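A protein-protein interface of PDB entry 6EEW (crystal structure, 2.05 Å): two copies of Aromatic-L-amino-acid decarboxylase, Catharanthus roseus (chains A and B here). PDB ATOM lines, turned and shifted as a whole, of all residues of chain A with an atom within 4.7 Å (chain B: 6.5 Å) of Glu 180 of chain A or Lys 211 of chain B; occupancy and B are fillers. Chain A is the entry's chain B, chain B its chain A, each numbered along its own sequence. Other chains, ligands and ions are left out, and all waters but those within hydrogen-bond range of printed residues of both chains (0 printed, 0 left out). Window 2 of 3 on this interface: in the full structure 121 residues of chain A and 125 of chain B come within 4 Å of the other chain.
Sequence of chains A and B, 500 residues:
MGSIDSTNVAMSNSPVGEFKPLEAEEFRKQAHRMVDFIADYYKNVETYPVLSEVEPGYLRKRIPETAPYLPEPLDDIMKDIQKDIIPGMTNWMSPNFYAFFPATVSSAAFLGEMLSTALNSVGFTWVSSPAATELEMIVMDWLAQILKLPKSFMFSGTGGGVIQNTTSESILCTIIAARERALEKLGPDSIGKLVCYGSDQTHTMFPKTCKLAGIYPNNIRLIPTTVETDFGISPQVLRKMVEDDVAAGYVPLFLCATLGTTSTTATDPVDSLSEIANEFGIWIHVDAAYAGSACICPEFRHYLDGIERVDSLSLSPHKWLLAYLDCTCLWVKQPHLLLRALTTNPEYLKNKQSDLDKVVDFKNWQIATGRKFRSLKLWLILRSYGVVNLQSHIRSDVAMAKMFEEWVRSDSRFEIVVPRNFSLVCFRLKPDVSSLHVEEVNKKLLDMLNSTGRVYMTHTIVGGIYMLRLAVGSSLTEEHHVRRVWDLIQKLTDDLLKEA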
ATOM      1  N   ILE A 176      -6.413  -6.679 -17.861  1.00  0.00           N
ATOM      2  CA  ILE A 176      -7.356  -7.498 -17.101  1.00  0.00           C
ATOM      3  C   ILE A 176      -7.395  -8.918 -17.660  1.00  0.00           C
ATOM      4  O   ILE A 176      -7.500  -9.891 -16.907  1.00  0.00           O
ATOM      5  CB  ILE A 176      -8.748  -6.836 -17.056  1.00  0.00           C
ATOM      6  CG1 ILE A 176      -8.675  -5.567 -16.211  1.00  0.00           C
ATOM      7  CG2 ILE A 176      -9.783  -7.774 -16.398  1.00  0.00           C
ATOM      8  CD1 ILE A 176      -9.930  -4.764 -16.205  1.00  0.00           C
ATOM      9  N   ALA A 177      -7.300  -9.066 -18.985  1.00  0.00           N
ATOM     10  CA  ALA A 177      -7.195 -10.405 -19.575  1.00  0.00           C
ATOM     11  C   ALA A 177      -6.011 -11.174 -18.995  1.00  0.00           C
ATOM     12  O   ALA A 177      -6.145 -12.329 -18.561  1.00  0.00           O
ATOM     13  CB  ALA A 177      -7.056 -10.309 -21.098  1.00  0.00           C
ATOM     14  N   ALA A 178      -4.838 -10.544 -18.982  1.00  0.00           N
ATOM     15  CA  ALA A 178      -3.656 -11.200 -18.425  1.00  0.00           C
ATOM     16  C   ALA A 178      -3.841 -11.515 -16.942  1.00  0.00           C
ATOM     17  O   ALA A 178      -3.516 -12.622 -16.480  1.00  0.00           O
ATOM     18  CB  ALA A 178      -2.434 -10.319 -18.641  1.00  0.00           C
ATOM     19  N   ARG A 179      -4.342 -10.538 -16.174  1.00  0.00           N
ATOM     20  CA  ARG A 179      -4.610 -10.755 -14.754  1.00  0.00           C
ATOM     21  C   ARG A 179      -5.532 -11.942 -14.543  1.00  0.00           C
ATOM     22  O   ARG A 179      -5.341 -12.730 -13.613  1.00  0.00           O
ATOM     23  CB  ARG A 179      -5.216  -9.498 -14.132  1.00  0.00           C
ATOM     24  CG  ARG A 179      -5.496  -9.598 -12.628  1.00  0.00           C
ATOM     25  CD  ARG A 179      -6.483  -8.521 -12.162  1.00  0.00           C
ATOM     26  NE  ARG A 179      -7.874  -8.819 -12.511  1.00  0.00           N
ATOM     27  CZ  ARG A 179      -8.861  -7.922 -12.500  1.00  0.00           C
ATOM     28  NH1 ARG A 179      -8.618  -6.657 -12.175  1.00  0.00           N
ATOM     29  NH2 ARG A 179     -10.097  -8.283 -12.830  1.00  0.00           N
ATOM     30  N   GLU A 180      -6.569 -12.060 -15.369  1.00  0.00           N
ATOM     31  CA  GLU A 180      -7.550 -13.118 -15.181  1.00  0.00           C
ATOM     32  C   GLU A 180      -6.976 -14.477 -15.547  1.00  0.00           C
ATOM     33  O   GLU A 180      -7.289 -15.474 -14.892  1.00  0.00           O
ATOM     34  CB  GLU A 180      -8.804 -12.806 -15.989  1.00  0.00           C
ATOM     35  CG  GLU A 180      -9.696 -11.803 -15.293  1.00  0.00           C
ATOM     36  CD  GLU A 180     -10.097 -12.248 -13.879  1.00  0.00           C
ATOM     37  OE1 GLU A 180     -10.372 -13.461 -13.674  1.00  0.00           O
ATOM     38  OE2 GLU A 180     -10.111 -11.380 -12.973  1.00  0.00           O
ATOM     39  N   ARG A 181      -6.135 -14.547 -16.586  1.00  0.00           N
ATOM     40  CA  ARG A 181      -5.426 -15.800 -16.854  1.00  0.00           C
ATOM     41  C   ARG A 181      -4.603 -16.229 -15.641  1.00  0.00           C
ATOM     42  O   ARG A 181      -4.666 -17.390 -15.190  1.00  0.00           O
ATOM     43  CB  ARG A 181      -4.531 -15.660 -18.085  1.00  0.00           C
ATOM     44  CG  ARG A 181      -3.760 -16.925 -18.387  1.00  0.00           C
ATOM     45  CD  ARG A 181      -3.010 -16.826 -19.690  1.00  0.00           C
ATOM     46  NE  ARG A 181      -2.062 -15.720 -19.680  1.00  0.00           N
ATOM     47  CZ  ARG A 181      -1.333 -15.353 -20.732  1.00  0.00           C
ATOM     48  NH1 ARG A 181      -1.441 -16.008 -21.881  1.00  0.00           N
ATOM     49  NH2 ARG A 181      -0.488 -14.331 -20.629  1.00  0.00           N
ATOM     50  N   ALA A 182      -3.833 -15.291 -15.083  1.00  0.00           N
ATOM     51  CA  ALA A 182      -3.046 -15.608 -13.895  1.00  0.00           C
ATOM     52  C   ALA A 182      -3.939 -16.039 -12.735  1.00  0.00           C
ATOM     53  O   ALA A 182      -3.679 -17.057 -12.085  1.00  0.00           O
ATOM     54  CB  ALA A 182      -2.186 -14.407 -13.501  1.00  0.00           C
ATOM     55  N   LEU A 183      -5.004 -15.283 -12.464  1.00  0.00           N
ATOM     56  CA  LEU A 183      -5.832 -15.569 -11.296  1.00  0.00           C
ATOM     57  C   LEU A 183      -6.548 -16.900 -11.434  1.00  0.00           C
ATOM     58  O   LEU A 183      -6.712 -17.622 -10.444  1.00  0.00           O
ATOM     59  CB  LEU A 183      -6.839 -14.449 -11.052  1.00  0.00           C
ATOM     60  CG  LEU A 183      -6.278 -13.070 -10.700  1.00  0.00           C
ATOM     61  CD1 LEU A 183      -7.418 -12.095 -10.459  1.00  0.00           C
ATOM     62  CD2 LEU A 183      -5.338 -13.153  -9.495  1.00  0.00           C
ATOM     63  N   GLU A 184      -6.991 -17.249 -12.644  1.00  0.00           N
ATOM     64  CA  GLU A 184      -7.627 -18.550 -12.798  1.00  0.00           C
ATOM     65  C   GLU A 184      -6.620 -19.678 -12.642  1.00  0.00           C
ATOM     66  O   GLU A 184      -6.966 -20.733 -12.095  1.00  0.00           O
ATOM     67  CB  GLU A 184      -8.359 -18.648 -14.135  1.00  0.00           C
ATOM     68  CG  GLU A 184      -9.587 -17.744 -14.201  1.00  0.00           C
ATOM     69  CD  GLU A 184     -10.429 -17.971 -15.443  1.00  0.00           C
ATOM     70  OE1 GLU A 184     -10.286 -19.030 -16.081  1.00  0.00           O
ATOM     71  OE2 GLU A 184     -11.242 -17.086 -15.776  1.00  0.00           O
ATOM     72  N   ARG A 340     -12.967 -14.350 -21.843  1.00  0.00           N
ATOM     73  CA  ARG A 340     -13.058 -14.901 -20.498  1.00  0.00           C
ATOM     74  C   ARG A 340     -12.884 -13.813 -19.449  1.00  0.00           C
ATOM     75  O   ARG A 340     -13.626 -13.769 -18.464  1.00  0.00           O
ATOM     76  CB  ARG A 340     -12.030 -16.014 -20.284  1.00  0.00           C
ATOM     77  CG  ARG A 340     -12.333 -17.308 -21.017  1.00  0.00           C
ATOM     78  CD  ARG A 340     -11.335 -18.412 -20.646  1.00  0.00           C
ATOM     79  NE  ARG A 340     -11.490 -18.883 -19.269  1.00  0.00           N
ATOM     80  CZ  ARG A 340     -12.374 -19.802 -18.882  1.00  0.00           C
ATOM     81  NH1 ARG A 340     -13.198 -20.353 -19.766  1.00  0.00           N
ATOM     82  NH2 ARG A 340     -12.444 -20.168 -17.606  1.00  0.00           N
ATOM     83  N   ALA A 341     -11.923 -12.910 -19.650  1.00  0.00           N
ATOM     84  CA  ALA A 341     -11.629 -11.936 -18.604  1.00  0.00           C
ATOM     85  C   ALA A 341     -12.818 -11.017 -18.332  1.00  0.00           C
ATOM     86  O   ALA A 341     -13.057 -10.626 -17.185  1.00  0.00           O
ATOM     87  CB  ALA A 341     -10.390 -11.122 -18.985  1.00  0.00           C
ATOM     88  N   THR A 343     -16.161 -11.330 -18.485  1.00  0.00           N
ATOM     89  CA  THR A 343     -17.497 -11.862 -18.252  1.00  0.00           C
ATOM     90  C   THR A 343     -17.527 -12.658 -16.957  1.00  0.00           C
ATOM     91  O   THR A 343     -16.499 -13.126 -16.464  1.00  0.00           O
ATOM     92  CB  THR A 343     -17.978 -12.736 -19.416  1.00  0.00           C
ATOM     93  OG1 THR A 343     -19.315 -13.187 -19.146  1.00  0.00           O
ATOM     94  CG2 THR A 343     -17.061 -13.934 -19.603  1.00  0.00           C
ATOM     95  N   THR A 344     -18.728 -12.782 -16.398  1.00  0.00           N
ATOM     96  CA  THR A 344     -18.962 -13.560 -15.187  1.00  0.00           C
ATOM     97  C   THR A 344     -19.680 -14.881 -15.457  1.00  0.00           C
ATOM     98  O   THR A 344     -20.488 -15.331 -14.640  1.00  0.00           O
ATOM     99  CB  THR A 344     -19.736 -12.720 -14.178  1.00  0.00           C
ATOM    100  OG1 THR A 344     -20.828 -12.073 -14.842  1.00  0.00           O
ATOM    101  CG2 THR A 344     -18.824 -11.667 -13.558  1.00  0.00           C
ATOM    102  N   PHE B 206     -23.463  -5.271 -13.595  1.00  0.00           N
ATOM    103  CA  PHE B 206     -22.863  -4.948 -12.301  1.00  0.00           C
ATOM    104  C   PHE B 206     -21.799  -5.955 -11.873  1.00  0.00           C
ATOM    105  O   PHE B 206     -20.702  -5.533 -11.460  1.00  0.00           O
ATOM    106  CB  PHE B 206     -23.991  -4.822 -11.271  1.00  0.00           C
ATOM    107  CG  PHE B 206     -23.540  -4.892  -9.855  1.00  0.00           C
ATOM    108  CD1 PHE B 206     -22.888  -3.824  -9.254  1.00  0.00           C
ATOM    109  CD2 PHE B 206     -23.737  -6.054  -9.135  1.00  0.00           C
ATOM    110  CE1 PHE B 206     -22.470  -3.915  -7.924  1.00  0.00           C
ATOM    111  CE2 PHE B 206     -23.323  -6.159  -7.810  1.00  0.00           C
ATOM    112  CZ  PHE B 206     -22.688  -5.087  -7.205  1.00  0.00           C
ATOM    113  N   PRO B 207     -22.040  -7.265 -11.920  1.00  0.00           N
ATOM    114  CA  PRO B 207     -20.967  -8.214 -11.572  1.00  0.00           C
ATOM    115  C   PRO B 207     -19.745  -8.102 -12.473  1.00  0.00           C
ATOM    116  O   PRO B 207     -18.602  -8.221 -12.004  1.00  0.00           O
ATOM    117  CB  PRO B 207     -21.653  -9.581 -11.718  1.00  0.00           C
ATOM    118  CG  PRO B 207     -23.153  -9.276 -11.600  1.00  0.00           C
ATOM    119  CD  PRO B 207     -23.321  -7.933 -12.217  1.00  0.00           C
ATOM    120  N   LYS B 208     -19.963  -7.924 -13.773  1.00  0.00           N
ATOM    121  CA  LYS B 208     -18.842  -7.736 -14.682  1.00  0.00           C
ATOM    122  C   LYS B 208     -17.980  -6.574 -14.218  1.00  0.00           C
ATOM    123  O   LYS B 208     -16.749  -6.677 -14.146  1.00  0.00           O
ATOM    124  CB  LYS B 208     -19.358  -7.494 -16.100  1.00  0.00           C
ATOM    125  CG  LYS B 208     -18.294  -7.022 -17.087  1.00  0.00           C
ATOM    126  CD  LYS B 208     -18.877  -6.875 -18.466  1.00  0.00           C
ATOM    127  CE  LYS B 208     -17.853  -6.353 -19.455  1.00  0.00           C
ATOM    128  NZ  LYS B 208     -18.427  -6.356 -20.828  1.00  0.00           N
ATOM    129  N   THR B 209     -18.624  -5.457 -13.891  1.00  0.00           N
ATOM    130  CA  THR B 209     -17.907  -4.291 -13.388  1.00  0.00           C
ATOM    131  C   THR B 209     -17.122  -4.626 -12.125  1.00  0.00           C
ATOM    132  O   THR B 209     -15.938  -4.295 -12.013  1.00  0.00           O
ATOM    133  CB  THR B 209     -18.891  -3.150 -13.134  1.00  0.00           C
ATOM    134  OG1 THR B 209     -19.396  -2.682 -14.390  1.00  0.00           O
ATOM    135  CG2 THR B 209     -18.195  -2.003 -12.443  1.00  0.00           C
ATOM    136  N   CYS B 210     -17.759  -5.301 -11.162  1.00  0.00           N
ATOM    137  CA  CYS B 210     -17.039  -5.656  -9.940  1.00  0.00           C
ATOM    138  C   CYS B 210     -15.799  -6.489 -10.259  1.00  0.00           C
ATOM    139  O   CYS B 210     -14.721  -6.263  -9.696  1.00  0.00           O
ATOM    140  CB  CYS B 210     -17.954  -6.419  -8.987  1.00  0.00           C
ATOM    141  SG  CYS B 210     -19.373  -5.451  -8.375  1.00  0.00           S
ATOM    142  N   LYS B 211     -15.942  -7.471 -11.148  1.00  0.00           N
ATOM    143  CA  LYS B 211     -14.808  -8.309 -11.518  1.00  0.00           C
ATOM    144  C   LYS B 211     -13.704  -7.470 -12.155  1.00  0.00           C
ATOM    145  O   LYS B 211     -12.516  -7.666 -11.868  1.00  0.00           O
ATOM    146  CB  LYS B 211     -15.273  -9.415 -12.467  1.00  0.00           C
ATOM    147  CG  LYS B 211     -14.175 -10.313 -12.992  1.00  0.00           C
ATOM    148  CD  LYS B 211     -14.719 -11.333 -13.988  1.00  0.00           C
ATOM    149  CE  LYS B 211     -13.623 -12.301 -14.406  1.00  0.00           C
ATOM    150  NZ  LYS B 211     -14.101 -13.371 -15.325  1.00  0.00           N
ATOM    151  N   LEU B 212     -14.080  -6.520 -13.016  1.00  0.00           N
ATOM    152  CA  LEU B 212     -13.088  -5.651 -13.634  1.00  0.00           C
ATOM    153  C   LEU B 212     -12.254  -4.914 -12.599  1.00  0.00           C
ATOM    154  O   LEU B 212     -11.068  -4.655 -12.835  1.00  0.00           O
ATOM    155  CB  LEU B 212     -13.761  -4.657 -14.574  1.00  0.00           C
ATOM    156  CG  LEU B 212     -14.440  -5.283 -15.792  1.00  0.00           C
ATOM    157  CD1 LEU B 212     -14.908  -4.202 -16.737  1.00  0.00           C
ATOM    158  CD2 LEU B 212     -13.478  -6.240 -16.506  1.00  0.00           C
ATOM    159  N   ALA B 213     -12.857  -4.541 -11.465  1.00  0.00           N
ATOM    160  CA  ALA B 213     -12.147  -3.805 -10.424  1.00  0.00           C
ATOM    161  C   ALA B 213     -11.312  -4.710  -9.535  1.00  0.00           C
ATOM    162  O   ALA B 213     -10.604  -4.203  -8.655  1.00  0.00           O
ATOM    163  CB  ALA B 213     -13.125  -3.012  -9.561  1.00  0.00           C
ATOM    164  N   GLY B 214     -11.373  -6.022  -9.742  1.00  0.00           N
ATOM    165  CA  GLY B 214     -10.606  -6.947  -8.947  1.00  0.00           C
ATOM    166  C   GLY B 214     -11.326  -7.519  -7.752  1.00  0.00           C
ATOM    167  O   GLY B 214     -10.696  -8.209  -6.941  1.00  0.00           O
ATOM    168  N   ILE B 215     -12.634  -7.286  -7.626  1.00  0.00           N
ATOM    169  CA  ILE B 215     -13.377  -7.904  -6.541  1.00  0.00           C
ATOM    170  C   ILE B 215     -13.299  -9.412  -6.700  1.00  0.00           C
ATOM    171  O   ILE B 215     -13.481  -9.942  -7.805  1.00  0.00           O
ATOM    172  CB  ILE B 215     -14.838  -7.419  -6.545  1.00  0.00           C
ATOM    173  CG1 ILE B 215     -14.908  -5.893  -6.601  1.00  0.00           C
ATOM    174  CG2 ILE B 215     -15.539  -7.862  -5.265  1.00  0.00           C
ATOM    175  CD1 ILE B 215     -14.375  -5.219  -5.352  1.00  0.00           C
ATOM    176  N   TYR B 216     -12.975 -10.113  -5.612  1.00  0.00           N
ATOM    177  CA  TYR B 216     -12.918 -11.560  -5.689  1.00  0.00           C
ATOM    178  C   TYR B 216     -14.262 -12.102  -6.172  1.00  0.00           C
ATOM    179  O   TYR B 216     -15.317 -11.540  -5.858  1.00  0.00           O
ATOM    180  CB  TYR B 216     -12.568 -12.165  -4.335  1.00  0.00           C
ATOM    181  CG  TYR B 216     -11.112 -12.071  -3.941  1.00  0.00           C
ATOM    182  CD1 TYR B 216     -10.272 -11.076  -4.451  1.00  0.00           C
ATOM    183  CD2 TYR B 216     -10.570 -12.993  -3.066  1.00  0.00           C
ATOM    184  CE1 TYR B 216      -8.928 -11.008  -4.076  1.00  0.00           C
ATOM    185  CE2 TYR B 216      -9.242 -12.937  -2.686  1.00  0.00           C
ATOM    186  CZ  TYR B 216      -8.418 -11.953  -3.191  1.00  0.00           C
ATOM    187  OH  TYR B 216      -7.087 -11.938  -2.792  1.00  0.00           O
ATOM    188  N   PRO B 217     -14.247 -13.183  -6.954  1.00  0.00           N
ATOM    189  CA  PRO B 217     -15.508 -13.724  -7.488  1.00  0.00           C
ATOM    190  C   PRO B 217     -16.574 -13.963  -6.433  1.00  0.00           C
ATOM    191  O   PRO B 217     -17.744 -13.620  -6.656  1.00  0.00           O
ATOM    192  CB  PRO B 217     -15.058 -15.034  -8.140  1.00  0.00           C
ATOM    193  CG  PRO B 217     -13.665 -14.730  -8.608  1.00  0.00           C
ATOM    194  CD  PRO B 217     -13.067 -13.812  -7.572  1.00  0.00           C
ATOM    195  N   ILE B 220     -18.839 -10.844  -4.760  1.00  0.00           N
ATOM    196  CA  ILE B 220     -19.844 -10.144  -5.551  1.00  0.00           C
ATOM    197  C   ILE B 220     -21.180 -10.794  -5.225  1.00  0.00           C
ATOM    198  O   ILE B 220     -21.395 -11.960  -5.570  1.00  0.00           O
ATOM    199  CB  ILE B 220     -19.540 -10.237  -7.051  1.00  0.00           C
ATOM    200  CG1 ILE B 220     -18.162  -9.649  -7.369  1.00  0.00           C
ATOM    201  CG2 ILE B 220     -20.612  -9.530  -7.860  1.00  0.00           C
ATOM    202  CD1 ILE B 220     -17.751  -9.782  -8.838  1.00  0.00           C
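O of Lys 211 of chain B lies within hydrogen-bond range of NH2 of Arg 179 of chain A (2.7 Å).
The backbone carbonyl oxygen of Arg 340 of chain A is in hydrogen-bond range of the side-chain amino group of Lys 211 of chain B (3.2 Å).
The backbone carbonyl oxygen of Ala 341 of chain A sits close to the side-chain amino group of Lys 211 of chain B (3.5 Å).
The side-chain amino group (NZ) of Lys 211 of chain B lies within hydrogen-bond range of the backbone carbonyl oxygen (O) of Thr 343 of chain A (2.7 Å).
O of Leu 212 of chain B sits at hydrogen-bond distance from NH1 of Arg 179 of chain A.
Printed residues of chain A that touch a printed residue of chain B: Ile 176, Arg 179, Glu 180, Arg 340, Ala 341, Thr 343 and Thr 344.
Hydrophobic or aromatic side chains of chain A within 4 Å of the printed part of chain B: Ile 176.
Along chain A the printed residues that touch a printed residue of chain B span positions 176 to 344.
Printed residues of chain B that touch a printed residue of chain A: Pro 207, Lys 208, Lys 211, Leu 212 and Gly 214.
Among the printed residues, no Asp or Glu carboxylate lies within 4 Å of a Lys or Arg side-chain nitrogen of the other chain.
Among the printed residues, pairs that only touch across the chains: Glu 180 of chain A with Lys 211 of chain B (3.5 Å), Ile 176 of chain A with Leu 212 of chain B (3.6 Å), Arg 179 of chain A with Gly 214 of chain B (3.7 Å), Thr 344 of chain A with Pro 207 of chain B (3.8 Å) and Thr 344 of chain A with Lys 208 of chain B (3.9 Å).
The side-chain carboxylate (OE2) of Glu 180 of chain A lies within salt-bridge range of the guanidinium group (NH2) of Arg 179 of chain A, 3.1 Å away.
OE1 of Glu 184 of chain A is in salt-bridge range of NH2 of Arg 340 of chain A, at 2.9 Å.
No position is printed for both chains.
Of the 10 pairs that touch across the chains among the printed residues, none has its exchanged pair printed and touching as well.
Of the printed residues of chain A, Pro 207 of chain B touches Thr 344.
Lys 211 of chain B touches five residues of chain A.
Ala 213 of chain B touches none of the printed residues of chain A.
Of the printed residues of chain A, Gly 214 of chain B touches Arg 179 (3.7 Å).
Pro 217 of chain B touches none of the printed residues of chain A.
The nearest residue of chain B that does not touch Glu 180 of chain A is Gly 214 of chain B (6.0 Å).
The nearest residue of chain A that does not touch Lys 211 of chain B is Thr 344 of chain A (4.1 Å).
The nearest printed residue of chain A that does not touch Leu 212 of chain B is Ala 341 of chain A (4.5 Å).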
